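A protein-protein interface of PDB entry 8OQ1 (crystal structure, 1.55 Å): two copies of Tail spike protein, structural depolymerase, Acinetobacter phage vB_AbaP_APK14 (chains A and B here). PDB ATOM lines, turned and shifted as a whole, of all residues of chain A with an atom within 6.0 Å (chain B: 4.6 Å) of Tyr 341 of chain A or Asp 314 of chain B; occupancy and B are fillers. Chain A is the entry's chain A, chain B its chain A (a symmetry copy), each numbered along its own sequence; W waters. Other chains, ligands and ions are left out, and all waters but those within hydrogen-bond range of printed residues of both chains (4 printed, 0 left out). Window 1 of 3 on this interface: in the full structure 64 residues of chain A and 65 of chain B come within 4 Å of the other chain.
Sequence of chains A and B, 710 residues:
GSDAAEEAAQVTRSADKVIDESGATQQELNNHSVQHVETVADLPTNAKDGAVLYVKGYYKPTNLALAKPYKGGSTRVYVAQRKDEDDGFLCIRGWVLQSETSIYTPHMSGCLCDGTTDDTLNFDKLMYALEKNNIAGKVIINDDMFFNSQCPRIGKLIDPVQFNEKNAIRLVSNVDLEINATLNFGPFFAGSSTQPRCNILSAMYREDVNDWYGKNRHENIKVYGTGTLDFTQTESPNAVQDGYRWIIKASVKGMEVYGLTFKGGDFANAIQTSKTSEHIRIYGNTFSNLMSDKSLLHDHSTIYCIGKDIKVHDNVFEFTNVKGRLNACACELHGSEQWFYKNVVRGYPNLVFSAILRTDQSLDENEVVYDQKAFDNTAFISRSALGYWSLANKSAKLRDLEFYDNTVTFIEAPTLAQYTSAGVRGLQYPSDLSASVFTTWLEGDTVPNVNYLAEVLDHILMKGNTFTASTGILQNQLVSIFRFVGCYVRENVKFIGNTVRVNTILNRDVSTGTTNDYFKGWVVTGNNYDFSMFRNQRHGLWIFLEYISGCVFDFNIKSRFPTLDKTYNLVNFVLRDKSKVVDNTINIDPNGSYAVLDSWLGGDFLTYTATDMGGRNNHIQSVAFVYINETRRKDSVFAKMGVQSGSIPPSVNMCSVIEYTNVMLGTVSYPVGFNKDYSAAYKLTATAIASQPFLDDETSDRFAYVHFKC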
ATOM      1  N   HIS A 279      28.809 -19.358  -9.457  1.00  0.00           N
ATOM      2  CA  HIS A 279      29.289 -18.066  -8.889  1.00  0.00           C
ATOM      3  C   HIS A 279      28.950 -16.944  -9.857  1.00  0.00           C
ATOM      4  O   HIS A 279      29.837 -16.319 -10.512  1.00  0.00           O
ATOM      5  CB  HIS A 279      30.777 -18.010  -8.624  1.00  0.00           C
ATOM      6  CG  HIS A 279      31.166 -16.954  -7.665  1.00  0.00           C
ATOM      7  ND1 HIS A 279      30.849 -16.981  -6.299  1.00  0.00           N
ATOM      8  CD2 HIS A 279      31.879 -15.821  -7.851  1.00  0.00           C
ATOM      9  CE1 HIS A 279      31.392 -15.939  -5.696  1.00  0.00           C
ATOM     10  NE2 HIS A 279      31.986 -15.185  -6.639  1.00  0.00           N
ATOM     11  N   ARG A 281      26.864 -13.301 -10.221  1.00  0.00           N
ATOM     12  CA  ARG A 281      26.319 -12.140  -9.502  1.00  0.00           C
ATOM     13  C   ARG A 281      25.699 -11.107 -10.441  1.00  0.00           C
ATOM     14  O   ARG A 281      26.386 -10.559 -11.302  1.00  0.00           O
ATOM     15  CB  ARG A 281      27.391 -11.466  -8.671  1.00  0.00           C
ATOM     16  CG  ARG A 281      28.075 -12.396  -7.688  1.00  0.00           C
ATOM     17  CD  ARG A 281      27.143 -12.741  -6.573  1.00  0.00           C
ATOM     18  NE  ARG A 281      27.722 -13.558  -5.496  1.00  0.00           N
ATOM     19  CZ  ARG A 281      27.848 -14.903  -5.502  1.00  0.00           C
ATOM     20  NH1 ARG A 281      27.371 -15.621  -6.507  1.00  0.00           N
ATOM     21  NH2 ARG A 281      28.278 -15.529  -4.407  1.00  0.00           N
ATOM     22  N   LYS A 311      23.399 -15.146  -7.372  1.00  0.00           N
ATOM     23  CA  LYS A 311      22.788 -14.072  -6.573  1.00  0.00           C
ATOM     24  C   LYS A 311      22.321 -12.933  -7.481  1.00  0.00           C
ATOM     25  O   LYS A 311      23.093 -12.339  -8.282  1.00  0.00           O
ATOM     26  CB  LYS A 311      23.690 -13.562  -5.459  1.00  0.00           C
ATOM     27  CG  LYS A 311      24.353 -14.653  -4.633  1.00  0.00           C
ATOM     28  CD  LYS A 311      23.430 -15.506  -3.883  1.00  0.00           C
ATOM     29  CE  LYS A 311      23.854 -16.960  -3.628  1.00  0.00           C
ATOM     30  NZ  LYS A 311      24.868 -17.063  -2.546  1.00  0.00           N
ATOM     31  N   VAL A 312      21.088 -12.670  -7.366  1.00  0.00           N
ATOM     32  CA  VAL A 312      20.365 -11.680  -8.204  1.00  0.00           C
ATOM     33  C   VAL A 312      19.785 -10.594  -7.293  1.00  0.00           C
ATOM     34  O   VAL A 312      18.833 -10.868  -6.540  1.00  0.00           O
ATOM     35  CB  VAL A 312      19.329 -12.298  -9.087  1.00  0.00           C
ATOM     36  CG1 VAL A 312      18.585 -11.267  -9.914  1.00  0.00           C
ATOM     37  CG2 VAL A 312      19.918 -13.414  -9.911  1.00  0.00           C
ATOM     38  N   HIS A 313      20.380  -9.449  -7.241  1.00  0.00           N
ATOM     39  CA  HIS A 313      20.015  -8.462  -6.206  1.00  0.00           C
ATOM     40  C   HIS A 313      20.034  -7.015  -6.686  1.00  0.00           C
ATOM     41  O   HIS A 313      20.849  -6.629  -7.558  1.00  0.00           O
ATOM     42  CB  HIS A 313      20.786  -8.734  -4.919  1.00  0.00           C
ATOM     43  CG  HIS A 313      22.239  -8.508  -5.078  1.00  0.00           C
ATOM     44  ND1 HIS A 313      22.875  -7.372  -4.570  1.00  0.00           N
ATOM     45  CD2 HIS A 313      23.214  -9.304  -5.538  1.00  0.00           C
ATOM     46  CE1 HIS A 313      24.141  -7.435  -4.844  1.00  0.00           C
ATOM     47  NE2 HIS A 313      24.399  -8.649  -5.303  1.00  0.00           N
ATOM     48  N   ASP A 314      19.305  -6.156  -6.003  1.00  0.00           N
ATOM     49  CA  ASP A 314      19.399  -4.670  -6.184  1.00  0.00           C
ATOM     50  C   ASP A 314      19.223  -4.322  -7.667  1.00  0.00           C
ATOM     51  O   ASP A 314      19.916  -3.470  -8.171  1.00  0.00           O
ATOM     52  CB  ASP A 314      20.736  -4.247  -5.521  1.00  0.00           C
ATOM     53  CG  ASP A 314      20.733  -4.464  -4.009  1.00  0.00           C
ATOM     54  OD1 ASP A 314      20.056  -3.640  -3.331  1.00  0.00           O
ATOM     55  OD2 ASP A 314      21.385  -5.420  -3.490  1.00  0.00           O
ATOM     56  N   ASN A 315      18.371  -5.050  -8.361  1.00  0.00           N
ATOM     57  CA  ASN A 315      17.992  -4.759  -9.758  1.00  0.00           C
ATOM     58  C   ASN A 315      16.607  -4.175  -9.828  1.00  0.00           C
ATOM     59  O   ASN A 315      15.771  -4.408  -8.909  1.00  0.00           O
ATOM     60  CB  ASN A 315      18.015  -5.975 -10.694  1.00  0.00           C
ATOM     61  CG  ASN A 315      19.366  -6.649 -10.651  1.00  0.00           C
ATOM     62  OD1 ASN A 315      20.382  -6.221 -11.251  1.00  0.00           O
ATOM     63  ND2 ASN A 315      19.410  -7.732  -9.962  1.00  0.00           N
ATOM     64  N   TRP A 339      19.853 -17.052  -4.841  1.00  0.00           N
ATOM     65  CA  TRP A 339      19.159 -16.026  -4.037  1.00  0.00           C
ATOM     66  C   TRP A 339      18.697 -14.849  -4.918  1.00  0.00           C
ATOM     67  O   TRP A 339      19.463 -14.300  -5.742  1.00  0.00           O
ATOM     68  CB  TRP A 339      19.895 -15.458  -2.842  1.00  0.00           C
ATOM     69  CG  TRP A 339      20.594 -16.451  -1.959  1.00  0.00           C
ATOM     70  CD1 TRP A 339      20.464 -17.784  -1.844  1.00  0.00           C
ATOM     71  CD2 TRP A 339      21.440 -16.033  -0.862  1.00  0.00           C
ATOM     72  NE1 TRP A 339      21.324 -18.239  -0.859  1.00  0.00           N
ATOM     73  CE2 TRP A 339      21.903 -17.203  -0.194  1.00  0.00           C
ATOM     74  CE3 TRP A 339      21.891 -14.807  -0.407  1.00  0.00           C
ATOM     75  CZ2 TRP A 339      22.784 -17.148   0.891  1.00  0.00           C
ATOM     76  CZ3 TRP A 339      22.751 -14.764   0.673  1.00  0.00           C
ATOM     77  CH2 TRP A 339      23.148 -15.933   1.375  1.00  0.00           C
ATOM     78  N   PHE A 340      17.539 -14.431  -4.626  1.00  0.00           N
ATOM     79  CA  PHE A 340      16.870 -13.295  -5.350  1.00  0.00           C
ATOM     80  C   PHE A 340      16.415 -12.295  -4.348  1.00  0.00           C
ATOM     81  O   PHE A 340      15.444 -12.591  -3.630  1.00  0.00           O
ATOM     82  CB  PHE A 340      15.752 -13.733  -6.286  1.00  0.00           C
ATOM     83  CG  PHE A 340      14.962 -12.686  -7.062  1.00  0.00           C
ATOM     84  CD1 PHE A 340      15.487 -12.130  -8.226  1.00  0.00           C
ATOM     85  CD2 PHE A 340      13.753 -12.265  -6.632  1.00  0.00           C
ATOM     86  CE1 PHE A 340      14.782 -11.202  -8.970  1.00  0.00           C
ATOM     87  CE2 PHE A 340      13.076 -11.239  -7.354  1.00  0.00           C
ATOM     88  CZ  PHE A 340      13.635 -10.695  -8.476  1.00  0.00           C
ATOM     89  N   TYR A 341      17.084 -11.187  -4.204  1.00  0.00           N
ATOM     90  CA  TYR A 341      16.886 -10.347  -2.990  1.00  0.00           C
ATOM     91  C   TYR A 341      17.116  -8.864  -3.239  1.00  0.00           C
ATOM     92  O   TYR A 341      17.927  -8.426  -4.115  1.00  0.00           O
ATOM     93  CB  TYR A 341      17.747 -10.779  -1.818  1.00  0.00           C
ATOM     94  CG  TYR A 341      19.217 -10.816  -2.087  1.00  0.00           C
ATOM     95  CD1 TYR A 341      19.836 -11.955  -2.635  1.00  0.00           C
ATOM     96  CD2 TYR A 341      20.040  -9.812  -1.572  1.00  0.00           C
ATOM     97  CE1 TYR A 341      21.216 -11.981  -2.855  1.00  0.00           C
ATOM     98  CE2 TYR A 341      21.399  -9.810  -1.855  1.00  0.00           C
ATOM     99  CZ  TYR A 341      21.999 -10.935  -2.385  1.00  0.00           C
ATOM    100  OH  TYR A 341      23.370 -10.933  -2.531  1.00  0.00           O
ATOM    101  N   LYS A 342      16.319  -8.056  -2.581  1.00  0.00           N
ATOM    102  CA  LYS A 342      16.463  -6.569  -2.618  1.00  0.00           C
ATOM    103  C   LYS A 342      16.218  -5.999  -4.026  1.00  0.00           C
ATOM    104  O   LYS A 342      16.824  -4.979  -4.410  1.00  0.00           O
ATOM    105  CB  LYS A 342      17.805  -6.125  -2.056  1.00  0.00           C
ATOM    106  CG  LYS A 342      17.927  -6.249  -0.577  1.00  0.00           C
ATOM    107  CD  LYS A 342      19.340  -5.862  -0.091  1.00  0.00           C
ATOM    108  CE  LYS A 342      19.475  -5.949   1.413  1.00  0.00           C
ATOM    109  NZ  LYS A 342      18.861  -7.186   1.961  1.00  0.00           N
ATOM    110  N   ASN A 343      15.423  -6.690  -4.830  1.00  0.00           N
ATOM    111  CA  ASN A 343      15.016  -6.195  -6.159  1.00  0.00           C
ATOM    112  C   ASN A 343      13.717  -5.418  -6.041  1.00  0.00           C
ATOM    113  O   ASN A 343      12.912  -5.665  -5.108  1.00  0.00           O
ATOM    114  CB  ASN A 343      14.879  -7.323  -7.168  1.00  0.00           C
ATOM    115  CG  ASN A 343      16.152  -8.142  -7.319  1.00  0.00           C
ATOM    116  OD1 ASN A 343      17.151  -7.730  -7.949  1.00  0.00           O
ATOM    117  ND2 ASN A 343      16.182  -9.262  -6.683  1.00  0.00           N
ATOM    118  N   LYS A 373      16.545 -18.923  -2.019  1.00  0.00           N
ATOM    119  CA  LYS A 373      16.061 -17.860  -1.074  1.00  0.00           C
ATOM    120  C   LYS A 373      15.574 -16.680  -1.862  1.00  0.00           C
ATOM    121  O   LYS A 373      16.313 -16.239  -2.778  1.00  0.00           O
ATOM    122  CB  LYS A 373      17.064 -17.385   0.000  1.00  0.00           C
ATOM    123  CG  LYS A 373      17.648 -18.565   0.722  1.00  0.00           C
ATOM    124  CD  LYS A 373      18.307 -18.203   2.138  1.00  0.00           C
ATOM    125  CE  LYS A 373      19.296 -17.096   2.039  1.00  0.00           C
ATOM    126  NZ  LYS A 373      20.289 -17.244   3.174  1.00  0.00           N
ATOM    127  N   ALA A 374      14.475 -16.080  -1.469  1.00  0.00           N
ATOM    128  CA  ALA A 374      13.962 -14.826  -2.057  1.00  0.00           C
ATOM    129  C   ALA A 374      13.464 -13.858  -0.986  1.00  0.00           C
ATOM    130  O   ALA A 374      12.579 -14.216  -0.159  1.00  0.00           O
ATOM    131  CB  ALA A 374      12.904 -15.062  -3.135  1.00  0.00           C
ATOM    132  N   PHE A 375      14.175 -12.769  -0.758  1.00  0.00           N
ATOM    133  CA  PHE A 375      13.945 -11.916   0.424  1.00  0.00           C
ATOM    134  C   PHE A 375      14.230 -10.429   0.182  1.00  0.00           C
ATOM    135  O   PHE A 375      14.995 -10.026  -0.676  1.00  0.00           O
ATOM    136  CB  PHE A 375      14.749 -12.461   1.631  1.00  0.00           C
ATOM    137  CG  PHE A 375      16.213 -12.494   1.365  1.00  0.00           C
ATOM    138  CD1 PHE A 375      16.791 -13.658   0.792  1.00  0.00           C
ATOM    139  CD2 PHE A 375      17.037 -11.512   1.890  1.00  0.00           C
ATOM    140  CE1 PHE A 375      18.161 -13.705   0.590  1.00  0.00           C
ATOM    141  CE2 PHE A 375      18.394 -11.567   1.632  1.00  0.00           C
ATOM    142  CZ  PHE A 375      18.959 -12.684   1.002  1.00  0.00           C
ATOM    143  N   ASP A 376      13.469  -9.609   0.841  1.00  0.00           N
ATOM    144  CA  ASP A 376      13.598  -8.135   0.905  1.00  0.00           C
ATOM    145  C   ASP A 376      13.214  -7.542  -0.467  1.00  0.00           C
ATOM    146  O   ASP A 376      13.674  -6.399  -0.749  1.00  0.00           O
ATOM    147  CB  ASP A 376      14.985  -7.681   1.367  1.00  0.00           C
ATOM    148  CG  ASP A 376      15.217  -7.845   2.862  1.00  0.00           C
ATOM    149  OD1 ASP A 376      14.323  -7.495   3.699  1.00  0.00           O
ATOM    150  OD2 ASP A 376      16.268  -8.439   3.198  1.00  0.00           O
ATOM    151  N   ASN A 377      12.490  -8.263  -1.339  1.00  0.00           N
ATOM    152  CA  ASN A 377      12.056  -7.716  -2.637  1.00  0.00           C
ATOM    153  C   ASN A 377      10.813  -6.842  -2.443  1.00  0.00           C
ATOM    154  O   ASN A 377       9.995  -7.025  -1.505  1.00  0.00           O
ATOM    155  CB  ASN A 377      11.773  -8.811  -3.677  1.00  0.00           C
ATOM    156  CG  ASN A 377      13.011  -9.618  -3.905  1.00  0.00           C
ATOM    157  OD1 ASN A 377      13.950  -9.219  -4.639  1.00  0.00           O
ATOM    158  ND2 ASN A 377      13.003 -10.823  -3.391  1.00  0.00           N
ATOM    159  N   TYR B 283      34.002  -8.928   1.638  1.00  0.00           N
ATOM    160  CA  TYR B 283      32.805  -9.322   0.842  1.00  0.00           C
ATOM    161  C   TYR B 283      33.122  -9.902  -0.542  1.00  0.00           C
ATOM    162  O   TYR B 283      34.170  -9.561  -1.165  1.00  0.00           O
ATOM    163  CB  TYR B 283      31.795  -8.147   0.804  1.00  0.00           C
ATOM    164  CG  TYR B 283      32.316  -7.000   0.014  1.00  0.00           C
ATOM    165  CD1 TYR B 283      33.025  -5.994   0.612  1.00  0.00           C
ATOM    166  CD2 TYR B 283      31.916  -6.823  -1.282  1.00  0.00           C
ATOM    167  CE1 TYR B 283      33.539  -4.940  -0.132  1.00  0.00           C
ATOM    168  CE2 TYR B 283      32.395  -5.773  -2.041  1.00  0.00           C
ATOM    169  CZ  TYR B 283      33.097  -4.746  -1.420  1.00  0.00           C
ATOM    170  OH  TYR B 283      33.531  -3.662  -2.163  1.00  0.00           O
ATOM    171  N   GLY B 284      32.254 -10.754  -1.062  1.00  0.00           N
ATOM    172  CA  GLY B 284      32.354 -11.337  -2.413  1.00  0.00           C
ATOM    173  C   GLY B 284      33.506 -12.294  -2.583  1.00  0.00           C
ATOM    174  O   GLY B 284      33.947 -12.550  -3.723  1.00  0.00           O
ATOM    175  N   ASN B 285      34.071 -12.792  -1.501  1.00  0.00           N
ATOM    176  CA  ASN B 285      35.246 -13.711  -1.593  1.00  0.00           C
ATOM    177  C   ASN B 285      34.807 -15.139  -1.471  1.00  0.00           C
ATOM    178  O   ASN B 285      33.684 -15.408  -0.935  1.00  0.00           O
ATOM    179  CB  ASN B 285      36.263 -13.366  -0.509  1.00  0.00           C
ATOM    180  CG  ASN B 285      36.661 -11.906  -0.499  1.00  0.00           C
ATOM    181  OD1 ASN B 285      37.475 -11.444  -1.325  1.00  0.00           O
ATOM    182  ND2 ASN B 285      36.246 -11.163   0.515  1.00  0.00           N
ATOM    183  N   HIS B 313      30.329 -10.056   4.576  1.00  0.00           N
ATOM    184  CA  HIS B 313      29.092 -10.362   3.830  1.00  0.00           C
ATOM    185  C   HIS B 313      29.325 -10.992   2.461  1.00  0.00           C
ATOM    186  O   HIS B 313      30.330 -10.698   1.771  1.00  0.00           O
ATOM    187  CB  HIS B 313      28.154  -9.160   3.845  1.00  0.00           C
ATOM    188  CG  HIS B 313      28.705  -8.010   3.095  1.00  0.00           C
ATOM    189  ND1 HIS B 313      28.240  -7.662   1.823  1.00  0.00           N
ATOM    190  CD2 HIS B 313      29.553  -7.039   3.458  1.00  0.00           C
ATOM    191  CE1 HIS B 313      28.888  -6.619   1.406  1.00  0.00           C
ATOM    192  NE2 HIS B 313      29.586  -6.138   2.423  1.00  0.00           N
ATOM    193  N   ASP B 314      28.330 -11.692   1.956  1.00  0.00           N
ATOM    194  CA  ASP B 314      28.298 -12.170   0.535  1.00  0.00           C
ATOM    195  C   ASP B 314      29.587 -12.940   0.223  1.00  0.00           C
ATOM    196  O   ASP B 314      30.136 -12.785  -0.842  1.00  0.00           O
ATOM    197  CB  ASP B 314      28.009 -10.914  -0.327  1.00  0.00           C
ATOM    198  CG  ASP B 314      26.618 -10.334  -0.070  1.00  0.00           C
ATOM    199  OD1 ASP B 314      25.649 -10.979  -0.561  1.00  0.00           O
ATOM    200  OD2 ASP B 314      26.474  -9.265   0.597  1.00  0.00           O
ATOM    201  N   ASN B 315      30.098 -13.678   1.188  1.00  0.00           N
ATOM    202  CA  ASN B 315      31.254 -14.578   1.006  1.00  0.00           C
ATOM    203  C   ASN B 315      30.814 -16.016   0.971  1.00  0.00           C
ATOM    204  O   ASN B 315      29.734 -16.365   1.528  1.00  0.00           O
ATOM    205  CB  ASN B 315      32.331 -14.464   2.094  1.00  0.00           C
ATOM    206  CG  ASN B 315      32.799 -13.034   2.224  1.00  0.00           C
ATOM    207  OD1 ASN B 315      33.602 -12.485   1.432  1.00  0.00           O
ATOM    208  ND2 ASN B 315      32.333 -12.401   3.239  1.00  0.00           N
ATOM    209  N   VAL B 316      31.647 -16.850   0.384  1.00  0.00           N
ATOM    210  CA  VAL B 316      31.458 -18.307   0.311  1.00  0.00           C
ATOM    211  C   VAL B 316      32.528 -18.813   1.228  1.00  0.00           C
ATOM    212  O   VAL B 316      33.686 -18.577   0.924  1.00  0.00           O
ATOM    213  CB  VAL B 316      31.573 -18.915  -1.113  1.00  0.00           C
ATOM    214  CG1 VAL B 316      31.713 -20.423  -1.111  1.00  0.00           C
ATOM    215  CG2 VAL B 316      30.411 -18.499  -2.041  1.00  0.00           C
ATOM    216  N   TYR B 341      26.752 -11.354   7.513  1.00  0.00           N
ATOM    217  CA  TYR B 341      25.419 -11.403   6.849  1.00  0.00           C
ATOM    218  C   TYR B 341      25.493 -11.782   5.378  1.00  0.00           C
ATOM    219  O   TYR B 341      26.493 -11.510   4.640  1.00  0.00           O
ATOM    220  CB  TYR B 341      24.642 -10.107   6.975  1.00  0.00           C
ATOM    221  CG  TYR B 341      25.341  -8.891   6.460  1.00  0.00           C
ATOM    222  CD1 TYR B 341      26.219  -8.148   7.269  1.00  0.00           C
ATOM    223  CD2 TYR B 341      24.948  -8.331   5.242  1.00  0.00           C
ATOM    224  CE1 TYR B 341      26.845  -6.998   6.778  1.00  0.00           C
ATOM    225  CE2 TYR B 341      25.621  -7.230   4.729  1.00  0.00           C
ATOM    226  CZ  TYR B 341      26.474  -6.502   5.534  1.00  0.00           C
ATOM    227  OH  TYR B 341      27.023  -5.346   5.023  1.00  0.00           O
ATOM    228  N   LYS B 342      24.509 -12.534   4.944  1.00  0.00           N
ATOM    229  CA  LYS B 342      24.356 -12.919   3.509  1.00  0.00           C
ATOM    230  C   LYS B 342      25.520 -13.799   3.018  1.00  0.00           C
ATOM    231  O   LYS B 342      25.904 -13.736   1.834  1.00  0.00           O
ATOM    232  CB  LYS B 342      24.160 -11.699   2.622  1.00  0.00           C
ATOM    233  CG  LYS B 342      22.824 -11.053   2.746  1.00  0.00           C
ATOM    234  CD  LYS B 342      22.730  -9.777   1.883  1.00  0.00           C
ATOM    235  CE  LYS B 342      21.369  -9.123   1.969  1.00  0.00           C
ATOM    236  NZ  LYS B 342      20.860  -9.064   3.363  1.00  0.00           N
ATOM    237  N   ASN B 343      26.145 -14.536   3.924  1.00  0.00           N
ATOM    238  CA  ASN B 343      27.198 -15.507   3.567  1.00  0.00           C
ATOM    239  C   ASN B 343      26.576 -16.871   3.327  1.00  0.00           C
ATOM    240  O   ASN B 343      25.495 -17.184   3.887  1.00  0.00           O
ATOM    241  CB  ASN B 343      28.281 -15.587   4.628  1.00  0.00           C
ATOM    242  CG  ASN B 343      28.932 -14.242   4.915  1.00  0.00           C
ATOM    243  OD1 ASN B 343      29.760 -13.713   4.142  1.00  0.00           O
ATOM    244  ND2 ASN B 343      28.517 -13.627   5.968  1.00  0.00           N
HETATM  245  O   HOH W   1      27.687 -16.190  -0.727  1.00  0.00           O
HETATM  246  O   HOH W   2      34.546 -15.149  -4.804  1.00  0.00           O
HETATM  247  O   HOH W   3      25.649 -14.904  -1.044  1.00  0.00           O
HETATM  248  O   HOH W   4      24.815  -8.745  -1.756  1.00  0.00           O
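Along chain A the printed residues that touch a printed residue of chain B span positions 339 to 375. Of the 10 printed residues of chain B, 3 touch a printed residue of chain A. Printed residues of chain B that touch a printed residue of chain A: Asp 314, Lys 342 and Asn 343. Among the printed residues, no Asp or Glu carboxylate lies within 4 Å of a Lys or Arg side-chain nitrogen of the other chain.
Printed residues of chain B within 4 Å of Tyr 341 of chain A: Asp 314 (3.0 Å) and Lys 342 (3.8 Å). Of the printed residues of chain A, Asp 314 of chain B touches Tyr 341. Of the printed residues of chain B, Trp 339 of chain A touches Lys 342 (3.5 Å) and Asn 343 (3.7 Å). Of the printed residues of chain B, Lys 342 of chain A touches Lys 342. Of the printed residues of chain A, Lys 342 of chain B touches Trp 339 (3.5 Å), Tyr 341 (3.8 Å), Lys 342 (3.1 Å) and Phe 375 (3.9 Å). Of the printed residues of chain B, Phe 375 of chain A touches Lys 342 (3.9 Å). Of the printed residues of chain A, Asn 343 of chain B touches Trp 339 (3.7 Å). Asp 376 of chain A touches none of the printed residues of chain B. Asn 285 of chain B touches none of the printed residues of chain A. The nearest printed residue of chain B that does not touch Tyr 341 of chain A is His 313 of chain B (7.3 Å).
The side-chain amino group of Lys 342 of chain B lies close to the side-chain amino group of Lys 342 of chain A (3.1 Å). OH of Tyr 341 of chain A is in hydrogen-bond range of OD1 of Asp 314 of chain B, 3.0 Å away.
Tyr 341 of chain A touches Asp 314 of chain B, but with the chains exchanged Asp 314 of chain A does not touch Tyr 341 of chain B (9.4 Å). Tyr 341 of chain A touches Lys 342 of chain B, but with the chains exchanged Lys 342 of chain A does not touch Tyr 341 of chain B (7.0 Å). Lys 342 of chain A touches its own counterpart, Lys 342 of chain B.
Lys 342 of chain B touches Trp 339 of chain A (O to CZ3, 3.5 Å). Trp 339 of chain A touches Asn 343 of chain B (CH2 to O, 3.7 Å). Lys 342 of chain B touches Tyr 341 of chain A (CE to CD2, 3.8 Å). Phe 375 of chain A touches Lys 342 of chain B.
N of Asn 315 of chain B lies within hydrogen-bond range of OD1 of Asn 343 of chain B, 3.0 Å away. The backbone carbonyl oxygen of Tyr 341 of chain A sits at hydrogen-bond distance from the side-chain amide nitrogen of Asn 343 of chain A (3.2 Å). The side-chain carboxylate (OD2) of Asp 314 of chain B sits at hydrogen-bond distance from a ring nitrogen (ND1) of His 313 of chain B, 2.7 Å away. The backbone carbonyl oxygen (O) of Val 312 of chain A is in hydrogen-bond range of the backbone NH (N) of Tyr 341 of chain A. The backbone NH of Val 312 of chain A lies within hydrogen-bond range of the backbone carbonyl oxygen of Trp 339 of chain A (2.8 Å). The backbone carbonyl oxygen (O) of Tyr 341 of chain B lies within hydrogen-bond range of the backbone NH (N) of Asp 314 of chain B.
Water W4 lies within hydrogen-bond range of OD1 of Asp 314 of chain B (2.7 Å) and OH of Tyr 341 of chain A (2.7 Å). Water W3 lies within hydrogen-bond range of the side-chain amino group of Lys 311 of chain A (2.7 Å) and the backbone carbonyl oxygen of Lys 342 of chain B (3.1 Å). Water W2 bridges O of Gly 284 of chain B and NE2 of His 279 of chain A. Water W1 lies within hydrogen-bond range of O of Asn 315 of chain B (3.1 Å) and NZ of Lys 311 of chain A (3.5 Å).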
